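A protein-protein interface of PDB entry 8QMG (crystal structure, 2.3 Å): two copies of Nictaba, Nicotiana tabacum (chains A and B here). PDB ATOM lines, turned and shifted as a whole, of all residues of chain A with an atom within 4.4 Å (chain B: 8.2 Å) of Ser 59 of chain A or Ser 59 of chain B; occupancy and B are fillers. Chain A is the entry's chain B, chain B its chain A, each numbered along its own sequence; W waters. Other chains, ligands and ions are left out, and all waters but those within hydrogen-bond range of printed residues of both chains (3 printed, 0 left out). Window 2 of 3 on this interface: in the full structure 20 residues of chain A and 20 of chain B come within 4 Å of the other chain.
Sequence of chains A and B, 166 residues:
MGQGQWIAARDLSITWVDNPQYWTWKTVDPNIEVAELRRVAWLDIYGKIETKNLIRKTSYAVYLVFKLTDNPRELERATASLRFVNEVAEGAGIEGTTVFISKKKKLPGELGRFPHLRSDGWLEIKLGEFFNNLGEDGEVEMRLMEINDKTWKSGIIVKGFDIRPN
OE1 of Glu 129 of chain B sits at hydrogen-bond distance from N of Phe 131 of chain A, at 3.2 Å.
The backbone NH (N) of Phe 131 of chain B is in hydrogen-bond range of the side-chain carboxylate (OE1) of Glu 129 of chain A (2.8 Å).
The side-chain hydroxyl (OG) of Ser 59 of chain B is in hydrogen-bond range of the side-chain amide nitrogen (ND2) of Asn 166 of chain B (2.7 Å).
The backbone NH of Tyr 60 of chain B sits at hydrogen-bond distance from the backbone carbonyl oxygen of Phe 130 of chain B.
OE2 of Glu 129 of chain B lies within salt-bridge range of NZ of Lys 126 of chain B (2.5 Å).
OG of Ser 59 of chain A is in hydrogen-bond range of OD1 of Asn 166 of chain A, at 2.9 Å.
ND2 of Asn 166 of chain A is in hydrogen-bond range of OE2 of Glu 129 of chain A, 3.2 Å away.
Among the printed residues, pairs that only touch across the chains: Asn 166 of chain A with Phe 131 of chain B, Phe 131 of chain A with Ser 59 of chain B, Glu 129 of chain A with Phe 130 of chain B, Phe 131 of chain A with Asn 166 of chain B, Ser 59 of chain A with Phe 131 of chain B and Ser 59 of chain A with Ser 59 of chain B.
Of the printed residues of chain B, Ser 59 of chain A touches Ser 59 and Phe 131.
Of the printed residues of chain B, Phe 131 of chain A touches Ser 59 (3.6 Å), Glu 129 (3.2 Å) and Asn 166 (3.6 Å).
Of the printed residues of chain A, Ser 59 of chain B touches Ser 59 (3.9 Å) and Phe 131 (3.6 Å).
Of the printed residues of chain A, Phe 130 of chain B touches Glu 129.
Arg 164 of chain B touches none of the printed residues of chain A.
Of the printed residues of chain A, Asn 166 of chain B touches Phe 131.
The nearest printed residue of chain A that does not touch Ser 59 of chain B is Thr 58 of chain A (6.0 Å).
Of the 10 printed residues of chain A, 4 touch a printed residue of chain B.
Printed residues of chain A that touch a printed residue of chain B: Ser 59, Glu 129, Phe 131 and Asn 166.
Printed residues of chain B that touch a printed residue of chain A: Ser 59, Glu 129, Phe 130, Phe 131 and Asn 166.
Among the printed residues, 8 pairs touch across the chains.
Among the printed residues, no Asp or Glu carboxylate lies within 4 Å of a Lys or Arg side-chain nitrogen of the other chain.
Ser 59 of chain B touches its own counterpart, Ser 59 of chain A.
Glu 129 of chain A touches Phe 130 of chain B, but with the chains exchanged Phe 130 of chain A does not touch Glu 129 of chain B (4.001 Å).
Glu 129 of chain A touches Phe 131 of chain B, and with the chains exchanged Phe 131 of chain A touches Glu 129 of chain B.
Phe 131 of chain A touches Asn 166 of chain B, and with the chains exchanged Asn 166 of chain A touches Phe 131 of chain B.
Water W3 lies within hydrogen-bond range of OE2 of Glu 129 of chain B, O of Phe 131 of chain A and NZ of Lys 126 of chain B.
Water W1 lies within hydrogen-bond range of NZ of Lys 57 of chain B and OXT of Asn 166 of chain A.
Water W2 bridges O of Phe 131 of chain B (3.0 Å) and OE2 of Glu 129 of chain A (3.2 Å).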
ATOM      1  N   THR A  58      -5.838  -8.337 -26.237  1.00  0.00           N
ATOM      2  CA  THR A  58      -5.662  -6.958 -25.802  1.00  0.00           C
ATOM      3  C   THR A  58      -6.433  -6.699 -24.513  1.00  0.00           C
ATOM      4  O   THR A  58      -7.555  -7.185 -24.328  1.00  0.00           O
ATOM      5  CB  THR A  58      -6.125  -5.974 -26.898  1.00  0.00           C
ATOM      6  OG1 THR A  58      -5.374  -6.195 -28.095  1.00  0.00           O
ATOM      7  CG2 THR A  58      -5.965  -4.534 -26.451  1.00  0.00           C
ATOM      8  N   SER A  59      -5.817  -5.925 -23.624  1.00  0.00           N
ATOM      9  CA  SER A  59      -6.460  -5.450 -22.408  1.00  0.00           C
ATOM     10  C   SER A  59      -7.137  -4.114 -22.691  1.00  0.00           C
ATOM     11  O   SER A  59      -6.522  -3.213 -23.265  1.00  0.00           O
ATOM     12  CB  SER A  59      -5.438  -5.288 -21.285  1.00  0.00           C
ATOM     13  OG  SER A  59      -6.069  -4.883 -20.080  1.00  0.00           O
ATOM     14  N   TYR A  60      -8.400  -3.996 -22.301  1.00  0.00           N
ATOM     15  CA  TYR A  60      -9.211  -2.825 -22.601  1.00  0.00           C
ATOM     16  C   TYR A  60      -9.694  -2.165 -21.315  1.00  0.00           C
ATOM     17  O   TYR A  60     -10.109  -2.845 -20.372  1.00  0.00           O
ATOM     18  CB  TYR A  60     -10.440  -3.203 -23.466  1.00  0.00           C
ATOM     19  CG  TYR A  60     -10.113  -3.569 -24.888  1.00  0.00           C
ATOM     20  CD1 TYR A  60      -9.908  -2.584 -25.842  1.00  0.00           C
ATOM     21  CD2 TYR A  60      -9.992  -4.898 -25.276  1.00  0.00           C
ATOM     22  CE1 TYR A  60      -9.584  -2.905 -27.148  1.00  0.00           C
ATOM     23  CE2 TYR A  60      -9.678  -5.230 -26.583  1.00  0.00           C
ATOM     24  CZ  TYR A  60      -9.472  -4.227 -27.514  1.00  0.00           C
ATOM     25  OH  TYR A  60      -9.156  -4.555 -28.818  1.00  0.00           O
ATOM     26  N   ALA A  61      -9.651  -0.837 -21.289  1.00  0.00           N
ATOM     27  CA  ALA A  61     -10.257  -0.038 -20.232  1.00  0.00           C
ATOM     28  C   ALA A  61     -11.483   0.680 -20.785  1.00  0.00           C
ATOM     29  O   ALA A  61     -11.512   1.071 -21.957  1.00  0.00           O
ATOM     30  CB  ALA A  61      -9.268   0.986 -19.674  1.00  0.00           C
ATOM     31  N   GLU A 129     -12.121  -2.787 -16.278  1.00  0.00           N
ATOM     32  CA  GLU A 129     -11.058  -3.294 -17.129  1.00  0.00           C
ATOM     33  C   GLU A 129     -11.334  -4.753 -17.443  1.00  0.00           C
ATOM     34  O   GLU A 129     -11.924  -5.478 -16.631  1.00  0.00           O
ATOM     35  CB  GLU A 129      -9.705  -3.155 -16.435  1.00  0.00           C
ATOM     36  CG  GLU A 129      -8.577  -2.721 -17.314  1.00  0.00           C
ATOM     37  CD  GLU A 129      -7.302  -2.542 -16.525  1.00  0.00           C
ATOM     38  OE1 GLU A 129      -6.672  -3.560 -16.157  1.00  0.00           O
ATOM     39  OE2 GLU A 129      -6.951  -1.383 -16.246  1.00  0.00           O
ATOM     40  N   PHE A 130     -10.902  -5.181 -18.628  1.00  0.00           N
ATOM     41  CA  PHE A 130     -11.086  -6.572 -19.016  1.00  0.00           C
ATOM     42  C   PHE A 130     -10.106  -6.925 -20.124  1.00  0.00           C
ATOM     43  O   PHE A 130      -9.712  -6.071 -20.914  1.00  0.00           O
ATOM     44  CB  PHE A 130     -12.534  -6.862 -19.477  1.00  0.00           C
ATOM     45  CG  PHE A 130     -12.908  -6.200 -20.780  1.00  0.00           C
ATOM     46  CD1 PHE A 130     -13.429  -4.921 -20.791  1.00  0.00           C
ATOM     47  CD2 PHE A 130     -12.736  -6.858 -21.983  1.00  0.00           C
ATOM     48  CE1 PHE A 130     -13.762  -4.302 -21.972  1.00  0.00           C
ATOM     49  CE2 PHE A 130     -13.062  -6.242 -23.176  1.00  0.00           C
ATOM     50  CZ  PHE A 130     -13.582  -4.961 -23.168  1.00  0.00           C
ATOM     51  N   PHE A 131      -9.757  -8.200 -20.198  1.00  0.00           N
ATOM     52  CA  PHE A 131      -8.905  -8.716 -21.258  1.00  0.00           C
ATOM     53  C   PHE A 131      -9.777  -9.372 -22.318  1.00  0.00           C
ATOM     54  O   PHE A 131     -10.620 -10.212 -22.001  1.00  0.00           O
ATOM     55  CB  PHE A 131      -7.885  -9.714 -20.697  1.00  0.00           C
ATOM     56  CG  PHE A 131      -6.919 -10.231 -21.721  1.00  0.00           C
ATOM     57  CD1 PHE A 131      -5.837  -9.462 -22.125  1.00  0.00           C
ATOM     58  CD2 PHE A 131      -7.104 -11.477 -22.297  1.00  0.00           C
ATOM     59  CE1 PHE A 131      -4.959  -9.924 -23.083  1.00  0.00           C
ATOM     60  CE2 PHE A 131      -6.219 -11.950 -23.250  1.00  0.00           C
ATOM     61  CZ  PHE A 131      -5.143 -11.166 -23.644  1.00  0.00           C
ATOM     62  N   ARG A 164     -11.099   1.716 -24.622  1.00  0.00           N
ATOM     63  CA  ARG A 164      -9.763   1.912 -25.161  1.00  0.00           C
ATOM     64  C   ARG A 164      -8.824   0.809 -24.702  1.00  0.00           C
ATOM     65  O   ARG A 164      -8.976   0.273 -23.598  1.00  0.00           O
ATOM     66  CB  ARG A 164      -9.174   3.262 -24.715  1.00  0.00           C
ATOM     67  CG  ARG A 164      -9.945   4.479 -25.164  1.00  0.00           C
ATOM     68  CD  ARG A 164      -9.059   5.728 -25.109  1.00  0.00           C
ATOM     69  NE  ARG A 164      -8.365   5.857 -23.832  1.00  0.00           N
ATOM     70  CZ  ARG A 164      -8.810   6.564 -22.806  1.00  0.00           C
ATOM     71  NH1 ARG A 164      -9.965   7.212 -22.859  1.00  0.00           N
ATOM     72  NH2 ARG A 164      -8.078   6.631 -21.702  1.00  0.00           N
ATOM     73  N   PRO A 165      -7.834   0.459 -25.525  1.00  0.00           N
ATOM     74  CA  PRO A 165      -6.771  -0.437 -25.047  1.00  0.00           C
ATOM     75  C   PRO A 165      -5.910   0.267 -24.010  1.00  0.00           C
ATOM     76  O   PRO A 165      -5.545   1.437 -24.169  1.00  0.00           O
ATOM     77  CB  PRO A 165      -5.960  -0.769 -26.311  1.00  0.00           C
ATOM     78  CG  PRO A 165      -6.802  -0.309 -27.476  1.00  0.00           C
ATOM     79  CD  PRO A 165      -7.685   0.802 -26.953  1.00  0.00           C
ATOM     80  N   ASN A 166      -5.579  -0.459 -22.947  1.00  0.00           N
ATOM     81  CA  ASN A 166      -4.676   0.065 -21.921  1.00  0.00           C
ATOM     82  C   ASN A 166      -3.333   0.448 -22.553  1.00  0.00           C
ATOM     83  O   ASN A 166      -2.997   0.026 -23.664  1.00  0.00           O
ATOM     84  CB  ASN A 166      -4.453  -0.951 -20.806  1.00  0.00           C
ATOM     85  CG  ASN A 166      -5.660  -1.099 -19.906  1.00  0.00           C
ATOM     86  OD1 ASN A 166      -6.439  -2.038 -20.038  1.00  0.00           O
ATOM     87  ND2 ASN A 166      -5.822  -0.169 -18.988  1.00  0.00           N
ATOM     88  OXT ASN A 166      -2.540   1.184 -21.967  1.00  0.00           O
ATOM     89  N   LEU B  54       6.600  -7.048 -11.802  1.00  0.00           N
ATOM     90  CA  LEU B  54       6.053  -7.743 -12.952  1.00  0.00           C
ATOM     91  C   LEU B  54       6.557  -7.127 -14.256  1.00  0.00           C
ATOM     92  O   LEU B  54       7.142  -6.039 -14.286  1.00  0.00           O
ATOM     93  CB  LEU B  54       4.528  -7.708 -12.911  1.00  0.00           C
ATOM     94  CG  LEU B  54       3.857  -8.302 -11.681  1.00  0.00           C
ATOM     95  CD1 LEU B  54       2.366  -7.993 -11.671  1.00  0.00           C
ATOM     96  CD2 LEU B  54       4.096  -9.803 -11.630  1.00  0.00           C
ATOM     97  N   ILE B  55       6.328  -7.850 -15.350  1.00  0.00           N
ATOM     98  CA  ILE B  55       6.665  -7.335 -16.669  1.00  0.00           C
ATOM     99  C   ILE B  55       5.725  -6.187 -17.008  1.00  0.00           C
ATOM    100  O   ILE B  55       4.505  -6.286 -16.821  1.00  0.00           O
ATOM    101  CB  ILE B  55       6.571  -8.450 -17.717  1.00  0.00           C
ATOM    102  CG1 ILE B  55       7.426  -9.642 -17.309  1.00  0.00           C
ATOM    103  CG2 ILE B  55       7.008  -7.936 -19.089  1.00  0.00           C
ATOM    104  CD1 ILE B  55       7.072 -10.926 -18.051  1.00  0.00           C
ATOM    105  N   ARG B  56       6.283  -5.091 -17.514  1.00  0.00           N
ATOM    106  CA  ARG B  56       5.476  -3.925 -17.833  1.00  0.00           C
ATOM    107  C   ARG B  56       4.660  -4.172 -19.094  1.00  0.00           C
ATOM    108  O   ARG B  56       4.937  -5.080 -19.874  1.00  0.00           O
ATOM    109  CB  ARG B  56       6.368  -2.695 -17.999  1.00  0.00           C
ATOM    110  CG  ARG B  56       6.923  -2.151 -16.677  1.00  0.00           C
ATOM    111  CD  ARG B  56       7.688  -0.849 -16.881  1.00  0.00           C
ATOM    112  NE  ARG B  56       8.983  -1.070 -17.506  1.00  0.00           N
ATOM    113  CZ  ARG B  56      10.136  -1.041 -16.853  1.00  0.00           C
ATOM    114  NH1 ARG B  56      10.186  -0.788 -15.553  1.00  0.00           N
ATOM    115  NH2 ARG B  56      11.264  -1.268 -17.519  1.00  0.00           N
ATOM    116  N   LYS B  57       3.618  -3.359 -19.266  1.00  0.00           N
ATOM    117  CA  LYS B  57       2.772  -3.401 -20.457  1.00  0.00           C
ATOM    118  C   LYS B  57       2.163  -4.785 -20.675  1.00  0.00           C
ATOM    119  O   LYS B  57       2.084  -5.281 -21.801  1.00  0.00           O
ATOM    120  CB  LYS B  57       3.565  -2.957 -21.690  1.00  0.00           C
ATOM    121  CG  LYS B  57       4.102  -1.528 -21.629  1.00  0.00           C
ATOM    122  CD  LYS B  57       2.986  -0.520 -21.411  1.00  0.00           C
ATOM    123  CE  LYS B  57       3.477   0.904 -21.640  1.00  0.00           C
ATOM    124  NZ  LYS B  57       2.364   1.913 -21.511  1.00  0.00           N
ATOM    125  N   THR B  58       1.714  -5.411 -19.594  1.00  0.00           N
ATOM    126  CA  THR B  58       1.252  -6.788 -19.654  1.00  0.00           C
ATOM    127  C   THR B  58       0.005  -6.942 -18.799  1.00  0.00           C
ATOM    128  O   THR B  58      -0.032  -6.471 -17.662  1.00  0.00           O
ATOM    129  CB  THR B  58       2.337  -7.761 -19.163  1.00  0.00           C
ATOM    130  OG1 THR B  58       3.507  -7.659 -19.986  1.00  0.00           O
ATOM    131  CG2 THR B  58       1.817  -9.197 -19.186  1.00  0.00           C
ATOM    132  N   SER B  59      -1.000  -7.623 -19.343  1.00  0.00           N
ATOM    133  CA  SER B  59      -2.206  -7.984 -18.609  1.00  0.00           C
ATOM    134  C   SER B  59      -1.986  -9.295 -17.869  1.00  0.00           C
ATOM    135  O   SER B  59      -1.459 -10.258 -18.432  1.00  0.00           O
ATOM    136  CB  SER B  59      -3.403  -8.119 -19.557  1.00  0.00           C
ATOM    137  OG  SER B  59      -4.486  -8.770 -18.909  1.00  0.00           O
ATOM    138  N   TYR B  60      -2.388  -9.322 -16.604  1.00  0.00           N
ATOM    139  CA  TYR B  60      -2.225 -10.487 -15.753  1.00  0.00           C
ATOM    140  C   TYR B  60      -3.584 -10.965 -15.253  1.00  0.00           C
ATOM    141  O   TYR B  60      -4.497 -10.174 -15.008  1.00  0.00           O
ATOM    142  CB  TYR B  60      -1.317 -10.181 -14.550  1.00  0.00           C
ATOM    143  CG  TYR B  60       0.150 -10.093 -14.886  1.00  0.00           C
ATOM    144  CD1 TYR B  60       0.953 -11.221 -14.844  1.00  0.00           C
ATOM    145  CD2 TYR B  60       0.735  -8.878 -15.255  1.00  0.00           C
ATOM    146  CE1 TYR B  60       2.314 -11.147 -15.158  1.00  0.00           C
ATOM    147  CE2 TYR B  60       2.081  -8.793 -15.565  1.00  0.00           C
ATOM    148  CZ  TYR B  60       2.861  -9.934 -15.516  1.00  0.00           C
ATOM    149  OH  TYR B  60       4.181  -9.856 -15.828  1.00  0.00           O
ATOM    150  N   ALA B  61      -3.712 -12.280 -15.107  1.00  0.00           N
ATOM    151  CA  ALA B  61      -4.859 -12.901 -14.460  1.00  0.00           C
ATOM    152  C   ALA B  61      -4.364 -13.649 -13.229  1.00  0.00           C
ATOM    153  O   ALA B  61      -3.263 -14.214 -13.243  1.00  0.00           O
ATOM    154  CB  ALA B  61      -5.584 -13.852 -15.412  1.00  0.00           C
ATOM    155  N   VAL B  62      -5.170 -13.648 -12.170  1.00  0.00           N
ATOM    156  CA  VAL B  62      -4.840 -14.315 -10.914  1.00  0.00           C
ATOM    157  C   VAL B  62      -5.880 -15.398 -10.658  1.00  0.00           C
ATOM    158  O   VAL B  62      -7.089 -15.136 -10.715  1.00  0.00           O
ATOM    159  CB  VAL B  62      -4.784 -13.322  -9.740  1.00  0.00           C
ATOM    160  CG1 VAL B  62      -4.481 -14.061  -8.442  1.00  0.00           C
ATOM    161  CG2 VAL B  62      -3.765 -12.263 -10.005  1.00  0.00           C
ATOM    162  N   LYS B 126     -10.762 -18.142 -11.517  1.00  0.00           N
ATOM    163  CA  LYS B 126     -10.177 -16.840 -11.800  1.00  0.00           C
ATOM    164  C   LYS B 126     -10.711 -15.807 -10.820  1.00  0.00           C
ATOM    165  O   LYS B 126     -11.921 -15.574 -10.752  1.00  0.00           O
ATOM    166  CB  LYS B 126     -10.502 -16.440 -13.235  1.00  0.00           C
ATOM    167  CG  LYS B 126      -9.857 -15.152 -13.719  1.00  0.00           C
ATOM    168  CD  LYS B 126     -10.584 -14.678 -14.974  1.00  0.00           C
ATOM    169  CE  LYS B 126      -9.616 -14.228 -16.045  1.00  0.00           C
ATOM    170  NZ  LYS B 126     -10.337 -13.958 -17.323  1.00  0.00           N
ATOM    171  N   GLY B 128      -9.649 -12.520 -10.801  1.00  0.00           N
ATOM    172  CA  GLY B 128      -9.724 -11.220 -11.437  1.00  0.00           C
ATOM    173  C   GLY B 128      -8.595 -11.027 -12.427  1.00  0.00           C
ATOM    174  O   GLY B 128      -7.738 -11.900 -12.625  1.00  0.00           O
ATOM    175  N   GLU B 129      -8.601  -9.840 -13.033  1.00  0.00           N
ATOM    176  CA  GLU B 129      -7.602  -9.438 -14.010  1.00  0.00           C
ATOM    177  C   GLU B 129      -7.169  -8.010 -13.721  1.00  0.00           C
ATOM    178  O   GLU B 129      -7.915  -7.233 -13.123  1.00  0.00           O
ATOM    179  CB  GLU B 129      -8.153  -9.525 -15.435  1.00  0.00           C
ATOM    180  CG  GLU B 129      -8.175 -10.915 -16.015  1.00  0.00           C
ATOM    181  CD  GLU B 129      -9.028 -11.003 -17.267  1.00  0.00           C
ATOM    182  OE1 GLU B 129      -9.800 -10.059 -17.535  1.00  0.00           O
ATOM    183  OE2 GLU B 129      -8.923 -12.026 -17.976  1.00  0.00           O
ATOM    184  N   PHE B 130      -5.957  -7.674 -14.153  1.00  0.00           N
ATOM    185  CA  PHE B 130      -5.476  -6.301 -14.073  1.00  0.00           C
ATOM    186  C   PHE B 130      -4.386  -6.114 -15.118  1.00  0.00           C
ATOM    187  O   PHE B 130      -3.715  -7.072 -15.512  1.00  0.00           O
ATOM    188  CB  PHE B 130      -4.955  -5.948 -12.674  1.00  0.00           C
ATOM    189  CG  PHE B 130      -3.714  -6.686 -12.277  1.00  0.00           C
ATOM    190  CD1 PHE B 130      -3.801  -7.956 -11.732  1.00  0.00           C
ATOM    191  CD2 PHE B 130      -2.464  -6.108 -12.434  1.00  0.00           C
ATOM    192  CE1 PHE B 130      -2.658  -8.647 -11.357  1.00  0.00           C
ATOM    193  CE2 PHE B 130      -1.319  -6.787 -12.060  1.00  0.00           C
ATOM    194  CZ  PHE B 130      -1.412  -8.056 -11.523  1.00  0.00           C
ATOM    195  N   PHE B 131      -4.232  -4.873 -15.571  1.00  0.00           N
ATOM    196  CA  PHE B 131      -3.178  -4.510 -16.504  1.00  0.00           C
ATOM    197  C   PHE B 131      -2.040  -3.845 -15.745  1.00  0.00           C
ATOM    198  O   PHE B 131      -2.266  -2.880 -15.006  1.00  0.00           O
ATOM    199  CB  PHE B 131      -3.707  -3.568 -17.579  1.00  0.00           C
ATOM    200  CG  PHE B 131      -2.687  -3.219 -18.629  1.00  0.00           C
ATOM    201  CD1 PHE B 131      -2.382  -4.115 -19.636  1.00  0.00           C
ATOM    202  CD2 PHE B 131      -2.038  -2.000 -18.612  1.00  0.00           C
ATOM    203  CE1 PHE B 131      -1.451  -3.800 -20.607  1.00  0.00           C
ATOM    204  CE2 PHE B 131      -1.111  -1.681 -19.580  1.00  0.00           C
ATOM    205  CZ  PHE B 131      -0.816  -2.582 -20.579  1.00  0.00           C
ATOM    206  N   ASN B 132      -0.829  -4.369 -15.915  1.00  0.00           N
ATOM    207  CA  ASN B 132       0.371  -3.744 -15.369  1.00  0.00           C
ATOM    208  C   ASN B 132       0.928  -2.819 -16.442  1.00  0.00           C
ATOM    209  O   ASN B 132       1.410  -3.286 -17.479  1.00  0.00           O
ATOM    210  CB  ASN B 132       1.408  -4.785 -14.958  1.00  0.00           C
ATOM    211  CG  ASN B 132       2.619  -4.163 -14.292  1.00  0.00           C
ATOM    212  OD1 ASN B 132       2.500  -3.181 -13.560  1.00  0.00           O
ATOM    213  ND2 ASN B 132       3.798  -4.717 -14.563  1.00  0.00           N
ATOM    214  N   ASN B 133       0.854  -1.514 -16.204  1.00  0.00           N
ATOM    215  CA  ASN B 133       1.331  -0.536 -17.171  1.00  0.00           C
ATOM    216  C   ASN B 133       2.833  -0.317 -17.024  1.00  0.00           C
ATOM    217  O   ASN B 133       3.635  -0.922 -17.745  1.00  0.00           O
ATOM    218  CB  ASN B 133       0.575   0.783 -17.000  1.00  0.00           C
ATOM    219  CG  ASN B 133       0.967   1.813 -18.032  1.00  0.00           C
ATOM    220  OD1 ASN B 133       1.386   1.477 -19.148  1.00  0.00           O
ATOM    221  ND2 ASN B 133       0.859   3.077 -17.658  1.00  0.00           N
ATOM    222  N   ILE B 163      -0.482 -16.443 -10.795  1.00  0.00           N
ATOM    223  CA  ILE B 163      -0.532 -15.151 -11.473  1.00  0.00           C
ATOM    224  C   ILE B 163       0.126 -15.329 -12.836  1.00  0.00           C
ATOM    225  O   ILE B 163       1.353 -15.460 -12.928  1.00  0.00           O
ATOM    226  CB  ILE B 163       0.168 -14.053 -10.668  1.00  0.00           C
ATOM    227  CG1 ILE B 163      -0.449 -13.918  -9.275  1.00  0.00           C
ATOM    228  CG2 ILE B 163       0.080 -12.716 -11.405  1.00  0.00           C
ATOM    229  CD1 ILE B 163       0.278 -14.696  -8.213  1.00  0.00           C
ATOM    230  N   ARG B 164      -0.681 -15.332 -13.893  1.00  0.00           N
ATOM    231  CA  ARG B 164      -0.195 -15.645 -15.222  1.00  0.00           C
ATOM    232  C   ARG B 164      -0.502 -14.512 -16.190  1.00  0.00           C
ATOM    233  O   ARG B 164      -1.575 -13.900 -16.108  1.00  0.00           O
ATOM    234  CB  ARG B 164      -0.834 -16.947 -15.747  1.00  0.00           C
ATOM    235  CG  ARG B 164      -0.669 -18.145 -14.819  1.00  0.00           C
ATOM    236  CD  ARG B 164      -0.979 -19.447 -15.531  1.00  0.00           C
ATOM    237  NE  ARG B 164      -2.339 -19.501 -16.054  1.00  0.00           N
ATOM    238  CZ  ARG B 164      -3.374 -19.992 -15.389  1.00  0.00           C
ATOM    239  NH1 ARG B 164      -3.249 -20.434 -14.149  1.00  0.00           N
ATOM    240  NH2 ARG B 164      -4.566 -20.037 -15.977  1.00  0.00           N
ATOM    241  N   PRO B 165       0.414 -14.203 -17.111  1.00  0.00           N
ATOM    242  CA  PRO B 165       0.086 -13.227 -18.159  1.00  0.00           C
ATOM    243  C   PRO B 165      -0.975 -13.790 -19.088  1.00  0.00           C
ATOM    244  O   PRO B 165      -0.931 -14.965 -19.463  1.00  0.00           O
ATOM    245  CB  PRO B 165       1.415 -13.013 -18.896  1.00  0.00           C
ATOM    246  CG  PRO B 165       2.474 -13.563 -17.975  1.00  0.00           C
ATOM    247  CD  PRO B 165       1.816 -14.664 -17.192  1.00  0.00           C
ATOM    248  N   ASN B 166      -1.928 -12.938 -19.461  1.00  0.00           N
ATOM    249  CA  ASN B 166      -3.001 -13.334 -20.369  1.00  0.00           C
ATOM    250  C   ASN B 166      -2.473 -13.519 -21.788  1.00  0.00           C
ATOM    251  O   ASN B 166      -1.517 -12.850 -22.193  1.00  0.00           O
ATOM    252  CB  ASN B 166      -4.126 -12.297 -20.361  1.00  0.00           C
ATOM    253  CG  ASN B 166      -5.038 -12.444 -19.164  1.00  0.00           C
ATOM    254  OD1 ASN B 166      -5.417 -13.555 -18.795  1.00  0.00           O
ATOM    255  ND2 ASN B 166      -5.393 -11.321 -18.543  1.00  0.00           N
ATOM    256  OXT ASN B 166      -2.994 -14.344 -22.553  1.00  0.00           O
HETATM  257  O   HOH W   1       0.328   0.739 -23.024  1.00  0.00           O
HETATM  258  O   HOH W   2      -4.291  -0.716 -14.645  1.00  0.00           O
HETATM  259  O   HOH W   3     -10.914 -11.815 -19.806  1.00  0.00           O
